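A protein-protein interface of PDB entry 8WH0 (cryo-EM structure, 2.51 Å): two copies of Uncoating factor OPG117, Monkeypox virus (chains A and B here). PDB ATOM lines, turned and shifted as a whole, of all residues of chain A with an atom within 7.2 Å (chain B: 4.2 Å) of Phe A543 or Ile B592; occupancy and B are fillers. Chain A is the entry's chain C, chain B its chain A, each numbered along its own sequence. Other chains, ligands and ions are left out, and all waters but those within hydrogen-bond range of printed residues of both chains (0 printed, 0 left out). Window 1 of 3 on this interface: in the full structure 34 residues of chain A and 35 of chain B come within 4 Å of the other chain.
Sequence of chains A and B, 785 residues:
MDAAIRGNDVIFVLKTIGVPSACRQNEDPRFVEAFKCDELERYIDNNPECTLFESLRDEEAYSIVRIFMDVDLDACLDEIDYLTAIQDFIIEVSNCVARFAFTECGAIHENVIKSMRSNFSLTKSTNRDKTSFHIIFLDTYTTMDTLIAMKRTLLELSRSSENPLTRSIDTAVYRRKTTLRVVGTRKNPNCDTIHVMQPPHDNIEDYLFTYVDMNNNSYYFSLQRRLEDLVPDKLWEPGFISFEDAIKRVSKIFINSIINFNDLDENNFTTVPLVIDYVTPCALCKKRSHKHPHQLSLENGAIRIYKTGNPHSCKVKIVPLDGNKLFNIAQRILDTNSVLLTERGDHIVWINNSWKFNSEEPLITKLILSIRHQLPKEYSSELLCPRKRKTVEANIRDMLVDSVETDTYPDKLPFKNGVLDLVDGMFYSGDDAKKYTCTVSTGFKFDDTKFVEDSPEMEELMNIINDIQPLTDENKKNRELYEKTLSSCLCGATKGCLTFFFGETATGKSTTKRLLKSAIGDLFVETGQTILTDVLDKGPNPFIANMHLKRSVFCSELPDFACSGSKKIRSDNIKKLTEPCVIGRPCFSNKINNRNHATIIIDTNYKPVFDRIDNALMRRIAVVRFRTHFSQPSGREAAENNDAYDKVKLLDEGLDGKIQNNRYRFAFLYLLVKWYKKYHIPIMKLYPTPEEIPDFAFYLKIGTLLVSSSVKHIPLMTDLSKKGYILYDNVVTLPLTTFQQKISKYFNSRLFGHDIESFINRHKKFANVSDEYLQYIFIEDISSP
Position printed for both chains: 585.
Among the printed residues, merely in contact across the chains: Glu A526 with Ile B583, Glu A526 with Ile B592, Thr A530 with Asp B537, Thr A530 with Lys B538, Pro A542 with Arg B585, Pro A542 with Asn B590, Pro A542 with Ile B592, Phe A543 with Asp B537, Phe A543 with Ile B583, Phe A543 with Ile B592 and Asn A546 with Asn B590.
N of Gly B584 lies within hydrogen-bond range of O of Ile B592 (2.6 Å). The side-chain amide oxygen (OD1) of Asn A546 lies close to the backbone carbonyl oxygen (O) of Pro A542 (3.0 Å).
Hydrophobic or aromatic side chains of chain B that line the printed part of chain A: Ile B583 and Ile B592.
Of the printed residues of chain B, Thr A530 touches Asp B537 (3.9 Å) and Lys B538 (3.9 Å). Of the printed residues of chain B, Pro A542 touches Arg B585, Asn B590 and Ile B592. Of chain B, only Asp B537 (3.8 Å), Ile B583 (3.4 Å) and Ile B592 (3.9 Å) come within 4 Å of Phe A543. Arg A585 touches none of the printed residues of chain B. Printed residues of chain A within 4 Å of Lys B538: Thr A530 (3.9 Å). Of the printed residues of chain A, Arg B585 touches Pro A542. The nearest residue of chain A that does not touch Ile B592 is Asn A546 (4.3 Å).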
ATOM      1  N   VAL A 525     -11.507  13.084  10.287  1.00  0.00           N
ATOM      2  CA  VAL A 525     -12.866  12.658   9.980  1.00  0.00           C
ATOM      3  C   VAL A 525     -12.858  11.813   8.714  1.00  0.00           C
ATOM      4  O   VAL A 525     -12.031  12.002   7.817  1.00  0.00           O
ATOM      5  CB  VAL A 525     -13.832  13.856   9.828  1.00  0.00           C
ATOM      6  CG1 VAL A 525     -13.690  14.490   8.458  1.00  0.00           C
ATOM      7  CG2 VAL A 525     -15.266  13.422  10.082  1.00  0.00           C
ATOM      8  N   GLU A 526     -13.787  10.866   8.658  1.00  0.00           N
ATOM      9  CA  GLU A 526     -14.007  10.020   7.495  1.00  0.00           C
ATOM     10  C   GLU A 526     -15.370  10.337   6.899  1.00  0.00           C
ATOM     11  O   GLU A 526     -16.350  10.499   7.631  1.00  0.00           O
ATOM     12  CB  GLU A 526     -13.940   8.539   7.874  1.00  0.00           C
ATOM     13  CG  GLU A 526     -12.745   7.796   7.323  1.00  0.00           C
ATOM     14  CD  GLU A 526     -12.699   6.359   7.801  1.00  0.00           C
ATOM     15  OE1 GLU A 526     -12.224   6.121   8.933  1.00  0.00           O
ATOM     16  OE2 GLU A 526     -13.143   5.466   7.050  1.00  0.00           O
ATOM     17  N   THR A 527     -15.434  10.430   5.574  1.00  0.00           N
ATOM     18  CA  THR A 527     -16.691  10.717   4.901  1.00  0.00           C
ATOM     19  C   THR A 527     -16.895   9.748   3.745  1.00  0.00           C
ATOM     20  O   THR A 527     -16.013   8.962   3.396  1.00  0.00           O
ATOM     21  CB  THR A 527     -16.748  12.166   4.394  1.00  0.00           C
ATOM     22  OG1 THR A 527     -15.455  12.563   3.922  1.00  0.00           O
ATOM     23  CG2 THR A 527     -17.192  13.101   5.505  1.00  0.00           C
ATOM     24  N   GLY A 528     -18.091   9.812   3.156  1.00  0.00           N
ATOM     25  CA  GLY A 528     -18.421   8.973   2.026  1.00  0.00           C
ATOM     26  C   GLY A 528     -18.082   9.620   0.697  1.00  0.00           C
ATOM     27  O   GLY A 528     -17.744  10.797   0.615  1.00  0.00           O
ATOM     28  N   GLN A 529     -18.185   8.818  -0.363  1.00  0.00           N
ATOM     29  CA  GLN A 529     -17.866   9.291  -1.704  1.00  0.00           C
ATOM     30  C   GLN A 529     -18.904  10.258  -2.257  1.00  0.00           C
ATOM     31  O   GLN A 529     -18.677  10.831  -3.326  1.00  0.00           O
ATOM     32  CB  GLN A 529     -17.707   8.104  -2.655  1.00  0.00           C
ATOM     33  CG  GLN A 529     -18.545   6.895  -2.284  1.00  0.00           C
ATOM     34  CD  GLN A 529     -18.190   5.669  -3.099  1.00  0.00           C
ATOM     35  OE1 GLN A 529     -17.043   5.219  -3.099  1.00  0.00           O
ATOM     36  NE2 GLN A 529     -19.174   5.120  -3.802  1.00  0.00           N
ATOM     37  N   THR A 530     -20.032  10.447  -1.568  1.00  0.00           N
ATOM     38  CA  THR A 530     -21.044  11.378  -2.055  1.00  0.00           C
ATOM     39  C   THR A 530     -20.466  12.777  -2.229  1.00  0.00           C
ATOM     40  O   THR A 530     -20.750  13.455  -3.223  1.00  0.00           O
ATOM     41  CB  THR A 530     -22.241  11.407  -1.105  1.00  0.00           C
ATOM     42  OG1 THR A 530     -21.784  11.320   0.251  1.00  0.00           O
ATOM     43  CG2 THR A 530     -23.178  10.248  -1.394  1.00  0.00           C
ATOM     44  N   ILE A 531     -19.638  13.220  -1.282  1.00  0.00           N
ATOM     45  CA  ILE A 531     -19.019  14.535  -1.361  1.00  0.00           C
ATOM     46  C   ILE A 531     -18.190  14.714  -2.623  1.00  0.00           C
ATOM     47  O   ILE A 531     -17.750  15.830  -2.912  1.00  0.00           O
ATOM     48  CB  ILE A 531     -18.147  14.794  -0.113  1.00  0.00           C
ATOM     49  CG1 ILE A 531     -16.822  14.039  -0.222  1.00  0.00           C
ATOM     50  CG2 ILE A 531     -18.892  14.398   1.150  1.00  0.00           C
ATOM     51  CD1 ILE A 531     -15.694  14.667   0.562  1.00  0.00           C
ATOM     52  N   PRO A 540     -30.531  18.452   4.128  1.00  0.00           N
ATOM     53  CA  PRO A 540     -29.749  18.136   5.334  1.00  0.00           C
ATOM     54  C   PRO A 540     -28.676  17.099   5.051  1.00  0.00           C
ATOM     55  O   PRO A 540     -28.986  15.949   4.728  1.00  0.00           O
ATOM     56  CB  PRO A 540     -30.804  17.604   6.314  1.00  0.00           C
ATOM     57  CG  PRO A 540     -32.099  18.145   5.830  1.00  0.00           C
ATOM     58  CD  PRO A 540     -31.983  18.352   4.349  1.00  0.00           C
ATOM     59  N   ASN A 541     -27.409  17.496   5.169  1.00  0.00           N
ATOM     60  CA  ASN A 541     -26.275  16.655   4.787  1.00  0.00           C
ATOM     61  C   ASN A 541     -25.295  16.549   5.947  1.00  0.00           C
ATOM     62  O   ASN A 541     -24.360  17.353   6.060  1.00  0.00           O
ATOM     63  CB  ASN A 541     -25.582  17.205   3.543  1.00  0.00           C
ATOM     64  CG  ASN A 541     -24.822  16.141   2.784  1.00  0.00           C
ATOM     65  OD1 ASN A 541     -24.957  14.950   3.063  1.00  0.00           O
ATOM     66  ND2 ASN A 541     -24.017  16.563   1.819  1.00  0.00           N
ATOM     67  N   PRO A 542     -25.481  15.571   6.835  1.00  0.00           N
ATOM     68  CA  PRO A 542     -24.482  15.357   7.896  1.00  0.00           C
ATOM     69  C   PRO A 542     -23.102  15.024   7.357  1.00  0.00           C
ATOM     70  O   PRO A 542     -22.097  15.364   7.996  1.00  0.00           O
ATOM     71  CB  PRO A 542     -25.067  14.194   8.712  1.00  0.00           C
ATOM     72  CG  PRO A 542     -26.498  14.093   8.313  1.00  0.00           C
ATOM     73  CD  PRO A 542     -26.630  14.658   6.940  1.00  0.00           C
ATOM     74  N   PHE A 543     -23.021  14.374   6.195  1.00  0.00           N
ATOM     75  CA  PHE A 543     -21.740  13.987   5.618  1.00  0.00           C
ATOM     76  C   PHE A 543     -20.892  15.181   5.210  1.00  0.00           C
ATOM     77  O   PHE A 543     -19.696  15.012   4.957  1.00  0.00           O
ATOM     78  CB  PHE A 543     -21.967  13.075   4.410  1.00  0.00           C
ATOM     79  CG  PHE A 543     -22.745  11.832   4.731  1.00  0.00           C
ATOM     80  CD1 PHE A 543     -22.102  10.691   5.177  1.00  0.00           C
ATOM     81  CD2 PHE A 543     -24.122  11.809   4.597  1.00  0.00           C
ATOM     82  CE1 PHE A 543     -22.816   9.549   5.478  1.00  0.00           C
ATOM     83  CE2 PHE A 543     -24.842  10.671   4.895  1.00  0.00           C
ATOM     84  CZ  PHE A 543     -24.189   9.538   5.337  1.00  0.00           C
ATOM     85  N   ILE A 544     -21.479  16.372   5.129  1.00  0.00           N
ATOM     86  CA  ILE A 544     -20.736  17.603   4.920  1.00  0.00           C
ATOM     87  C   ILE A 544     -20.679  18.440   6.191  1.00  0.00           C
ATOM     88  O   ILE A 544     -19.668  19.088   6.466  1.00  0.00           O
ATOM     89  CB  ILE A 544     -21.334  18.416   3.753  1.00  0.00           C
ATOM     90  CG1 ILE A 544     -20.881  17.839   2.410  1.00  0.00           C
ATOM     91  CG2 ILE A 544     -20.939  19.879   3.868  1.00  0.00           C
ATOM     92  CD1 ILE A 544     -19.462  18.198   2.040  1.00  0.00           C
ATOM     93  N   ALA A 545     -21.756  18.434   6.979  1.00  0.00           N
ATOM     94  CA  ALA A 545     -21.776  19.180   8.230  1.00  0.00           C
ATOM     95  C   ALA A 545     -20.757  18.658   9.230  1.00  0.00           C
ATOM     96  O   ALA A 545     -20.369  19.395  10.143  1.00  0.00           O
ATOM     97  CB  ALA A 545     -23.175  19.140   8.842  1.00  0.00           C
ATOM     98  N   ASN A 546     -20.315  17.411   9.087  1.00  0.00           N
ATOM     99  CA  ASN A 546     -19.326  16.850   9.999  1.00  0.00           C
ATOM    100  C   ASN A 546     -17.899  17.240   9.638  1.00  0.00           C
ATOM    101  O   ASN A 546     -16.974  16.888  10.376  1.00  0.00           O
ATOM    102  CB  ASN A 546     -19.451  15.325  10.036  1.00  0.00           C
ATOM    103  CG  ASN A 546     -20.437  14.850  11.080  1.00  0.00           C
ATOM    104  OD1 ASN A 546     -21.637  15.100  10.978  1.00  0.00           O
ATOM    105  ND2 ASN A 546     -19.934  14.164  12.097  1.00  0.00           N
ATOM    106  N   MET A 547     -17.703  17.956   8.535  1.00  0.00           N
ATOM    107  CA  MET A 547     -16.387  18.391   8.089  1.00  0.00           C
ATOM    108  C   MET A 547     -16.001  19.758   8.635  1.00  0.00           C
ATOM    109  O   MET A 547     -14.917  20.254   8.317  1.00  0.00           O
ATOM    110  CB  MET A 547     -16.344  18.423   6.559  1.00  0.00           C
ATOM    111  CG  MET A 547     -16.194  17.062   5.906  1.00  0.00           C
ATOM    112  SD  MET A 547     -16.029  17.173   4.114  1.00  0.00           S
ATOM    113  CE  MET A 547     -14.773  18.440   3.970  1.00  0.00           C
ATOM    114  N   VAL A 553      -9.729  15.141   6.274  1.00  0.00           N
ATOM    115  CA  VAL A 553     -10.911  14.434   5.798  1.00  0.00           C
ATOM    116  C   VAL A 553     -10.456  13.325   4.862  1.00  0.00           C
ATOM    117  O   VAL A 553      -9.687  13.573   3.925  1.00  0.00           O
ATOM    118  CB  VAL A 553     -11.898  15.377   5.085  1.00  0.00           C
ATOM    119  CG1 VAL A 553     -13.033  14.583   4.463  1.00  0.00           C
ATOM    120  CG2 VAL A 553     -12.439  16.412   6.058  1.00  0.00           C
ATOM    121  N   ARG A 585     -25.909  21.218   6.192  1.00  0.00           N
ATOM    122  CA  ARG A 585     -26.562  21.448   7.467  1.00  0.00           C
ATOM    123  C   ARG A 585     -26.976  20.131   8.108  1.00  0.00           C
ATOM    124  O   ARG A 585     -27.364  19.189   7.408  1.00  0.00           O
ATOM    125  CB  ARG A 585     -27.787  22.355   7.274  1.00  0.00           C
ATOM    126  CG  ARG A 585     -28.777  22.355   8.419  1.00  0.00           C
ATOM    127  CD  ARG A 585     -30.007  23.168   8.057  1.00  0.00           C
ATOM    128  NE  ARG A 585     -30.911  22.451   7.167  1.00  0.00           N
ATOM    129  CZ  ARG A 585     -31.875  21.636   7.573  1.00  0.00           C
ATOM    130  NH1 ARG A 585     -32.081  21.395   8.858  1.00  0.00           N
ATOM    131  NH2 ARG A 585     -32.654  21.050   6.669  1.00  0.00           N
ATOM    132  N   ASP B 537     -23.705   5.366   1.379  1.00  0.00           N
ATOM    133  CA  ASP B 537     -23.807   6.712   1.944  1.00  0.00           C
ATOM    134  C   ASP B 537     -25.172   7.331   1.654  1.00  0.00           C
ATOM    135  O   ASP B 537     -25.965   7.561   2.571  1.00  0.00           O
ATOM    136  CB  ASP B 537     -22.677   7.593   1.401  1.00  0.00           C
ATOM    137  N   LYS B 538     -25.460   7.592   0.375  1.00  0.00           N
ATOM    138  CA  LYS B 538     -26.756   8.089  -0.082  1.00  0.00           C
ATOM    139  C   LYS B 538     -27.446   8.967   0.956  1.00  0.00           C
ATOM    140  O   LYS B 538     -26.917  10.010   1.352  1.00  0.00           O
ATOM    141  CB  LYS B 538     -27.666   6.918  -0.460  1.00  0.00           C
ATOM    142  N   VAL B 582     -17.611   1.940   9.180  1.00  0.00           N
ATOM    143  CA  VAL B 582     -18.482   1.966   8.010  1.00  0.00           C
ATOM    144  C   VAL B 582     -19.326   3.231   8.070  1.00  0.00           C
ATOM    145  O   VAL B 582     -19.891   3.556   9.118  1.00  0.00           O
ATOM    146  CB  VAL B 582     -19.369   0.710   7.929  1.00  0.00           C
ATOM    147  CG1 VAL B 582     -20.229   0.750   6.681  1.00  0.00           C
ATOM    148  CG2 VAL B 582     -18.511  -0.542   7.942  1.00  0.00           C
ATOM    149  N   ILE B 583     -19.413   3.938   6.951  1.00  0.00           N
ATOM    150  CA  ILE B 583     -20.086   5.232   6.902  1.00  0.00           C
ATOM    151  C   ILE B 583     -21.546   5.030   6.520  1.00  0.00           C
ATOM    152  O   ILE B 583     -21.855   4.415   5.492  1.00  0.00           O
ATOM    153  CB  ILE B 583     -19.381   6.181   5.918  1.00  0.00           C
ATOM    154  CG1 ILE B 583     -17.909   6.340   6.300  1.00  0.00           C
ATOM    155  CG2 ILE B 583     -20.069   7.532   5.896  1.00  0.00           C
ATOM    156  CD1 ILE B 583     -17.695   7.058   7.606  1.00  0.00           C
ATOM    157  N   GLY B 584     -22.446   5.551   7.351  1.00  0.00           N
ATOM    158  CA  GLY B 584     -23.876   5.455   7.133  1.00  0.00           C
ATOM    159  C   GLY B 584     -24.646   5.889   8.363  1.00  0.00           C
ATOM    160  O   GLY B 584     -24.160   5.723   9.484  1.00  0.00           O
ATOM    161  N   ARG B 585     -25.842   6.439   8.182  1.00  0.00           N
ATOM    162  CA  ARG B 585     -26.593   6.975   9.304  1.00  0.00           C
ATOM    163  C   ARG B 585     -28.022   6.457   9.297  1.00  0.00           C
ATOM    164  O   ARG B 585     -28.556   6.100   8.245  1.00  0.00           O
ATOM    165  CB  ARG B 585     -26.614   8.511   9.279  1.00  0.00           C
ATOM    166  CG  ARG B 585     -27.187   9.104   8.004  1.00  0.00           C
ATOM    167  CD  ARG B 585     -27.649  10.533   8.225  1.00  0.00           C
ATOM    168  NE  ARG B 585     -28.364  11.061   7.070  1.00  0.00           N
ATOM    169  CZ  ARG B 585     -29.601  11.538   7.110  1.00  0.00           C
ATOM    170  NH1 ARG B 585     -30.292  11.568   8.236  1.00  0.00           N
ATOM    171  NH2 ARG B 585     -30.156  11.994   5.992  1.00  0.00           N
ATOM    172  N   ASN B 590     -27.453  12.097  13.196  1.00  0.00           N
ATOM    173  CA  ASN B 590     -26.261  12.731  12.654  1.00  0.00           C
ATOM    174  C   ASN B 590     -25.020  11.859  12.789  1.00  0.00           C
ATOM    175  O   ASN B 590     -23.955  12.241  12.294  1.00  0.00           O
ATOM    176  CB  ASN B 590     -26.015  14.079  13.339  1.00  0.00           C
ATOM    177  CG  ASN B 590     -27.058  15.114  12.981  1.00  0.00           C
ATOM    178  OD1 ASN B 590     -27.394  15.293  11.811  1.00  0.00           O
ATOM    179  ND2 ASN B 590     -27.578  15.806  13.988  1.00  0.00           N
ATOM    180  N   LYS B 591     -25.133  10.706  13.443  1.00  0.00           N
ATOM    181  CA  LYS B 591     -24.006   9.799  13.624  1.00  0.00           C
ATOM    182  C   LYS B 591     -23.798   9.017  12.333  1.00  0.00           C
ATOM    183  O   LYS B 591     -24.607   8.150  11.988  1.00  0.00           O
ATOM    184  CB  LYS B 591     -24.264   8.868  14.803  1.00  0.00           C
ATOM    185  CG  LYS B 591     -24.612   9.594  16.089  1.00  0.00           C
ATOM    186  CD  LYS B 591     -25.312   8.678  17.074  1.00  0.00           C
ATOM    187  CE  LYS B 591     -25.212   9.220  18.489  1.00  0.00           C
ATOM    188  NZ  LYS B 591     -26.251   8.646  19.388  1.00  0.00           N
ATOM    189  N   ILE B 592     -22.709   9.315  11.622  1.00  0.00           N
ATOM    190  CA  ILE B 592     -22.505   8.785  10.277  1.00  0.00           C
ATOM    191  C   ILE B 592     -21.499   7.644  10.222  1.00  0.00           C
ATOM    192  O   ILE B 592     -21.352   7.022   9.157  1.00  0.00           O
ATOM    193  CB  ILE B 592     -22.072   9.900   9.303  1.00  0.00           C
ATOM    194  CG1 ILE B 592     -20.796  10.578   9.803  1.00  0.00           C
ATOM    195  CG2 ILE B 592     -23.187  10.915   9.128  1.00  0.00           C
ATOM    196  CD1 ILE B 592     -19.964  11.193   8.706  1.00  0.00           C
ATOM    197  N   ASN B 593     -20.806   7.345  11.316  1.00  0.00           N
ATOM    198  CA  ASN B 593     -19.800   6.292  11.335  1.00  0.00           C
ATOM    199  C   ASN B 593     -20.188   5.231  12.352  1.00  0.00           C
ATOM    200  O   ASN B 593     -20.590   5.555  13.473  1.00  0.00           O
ATOM    201  CB  ASN B 593     -18.413   6.858  11.653  1.00  0.00           C
ATOM    202  CG  ASN B 593     -18.323   7.437  13.045  1.00  0.00           C
ATOM    203  OD1 ASN B 593     -19.322   7.875  13.614  1.00  0.00           O
ATOM    204  ND2 ASN B 593     -17.120   7.442  13.604  1.00  0.00           N
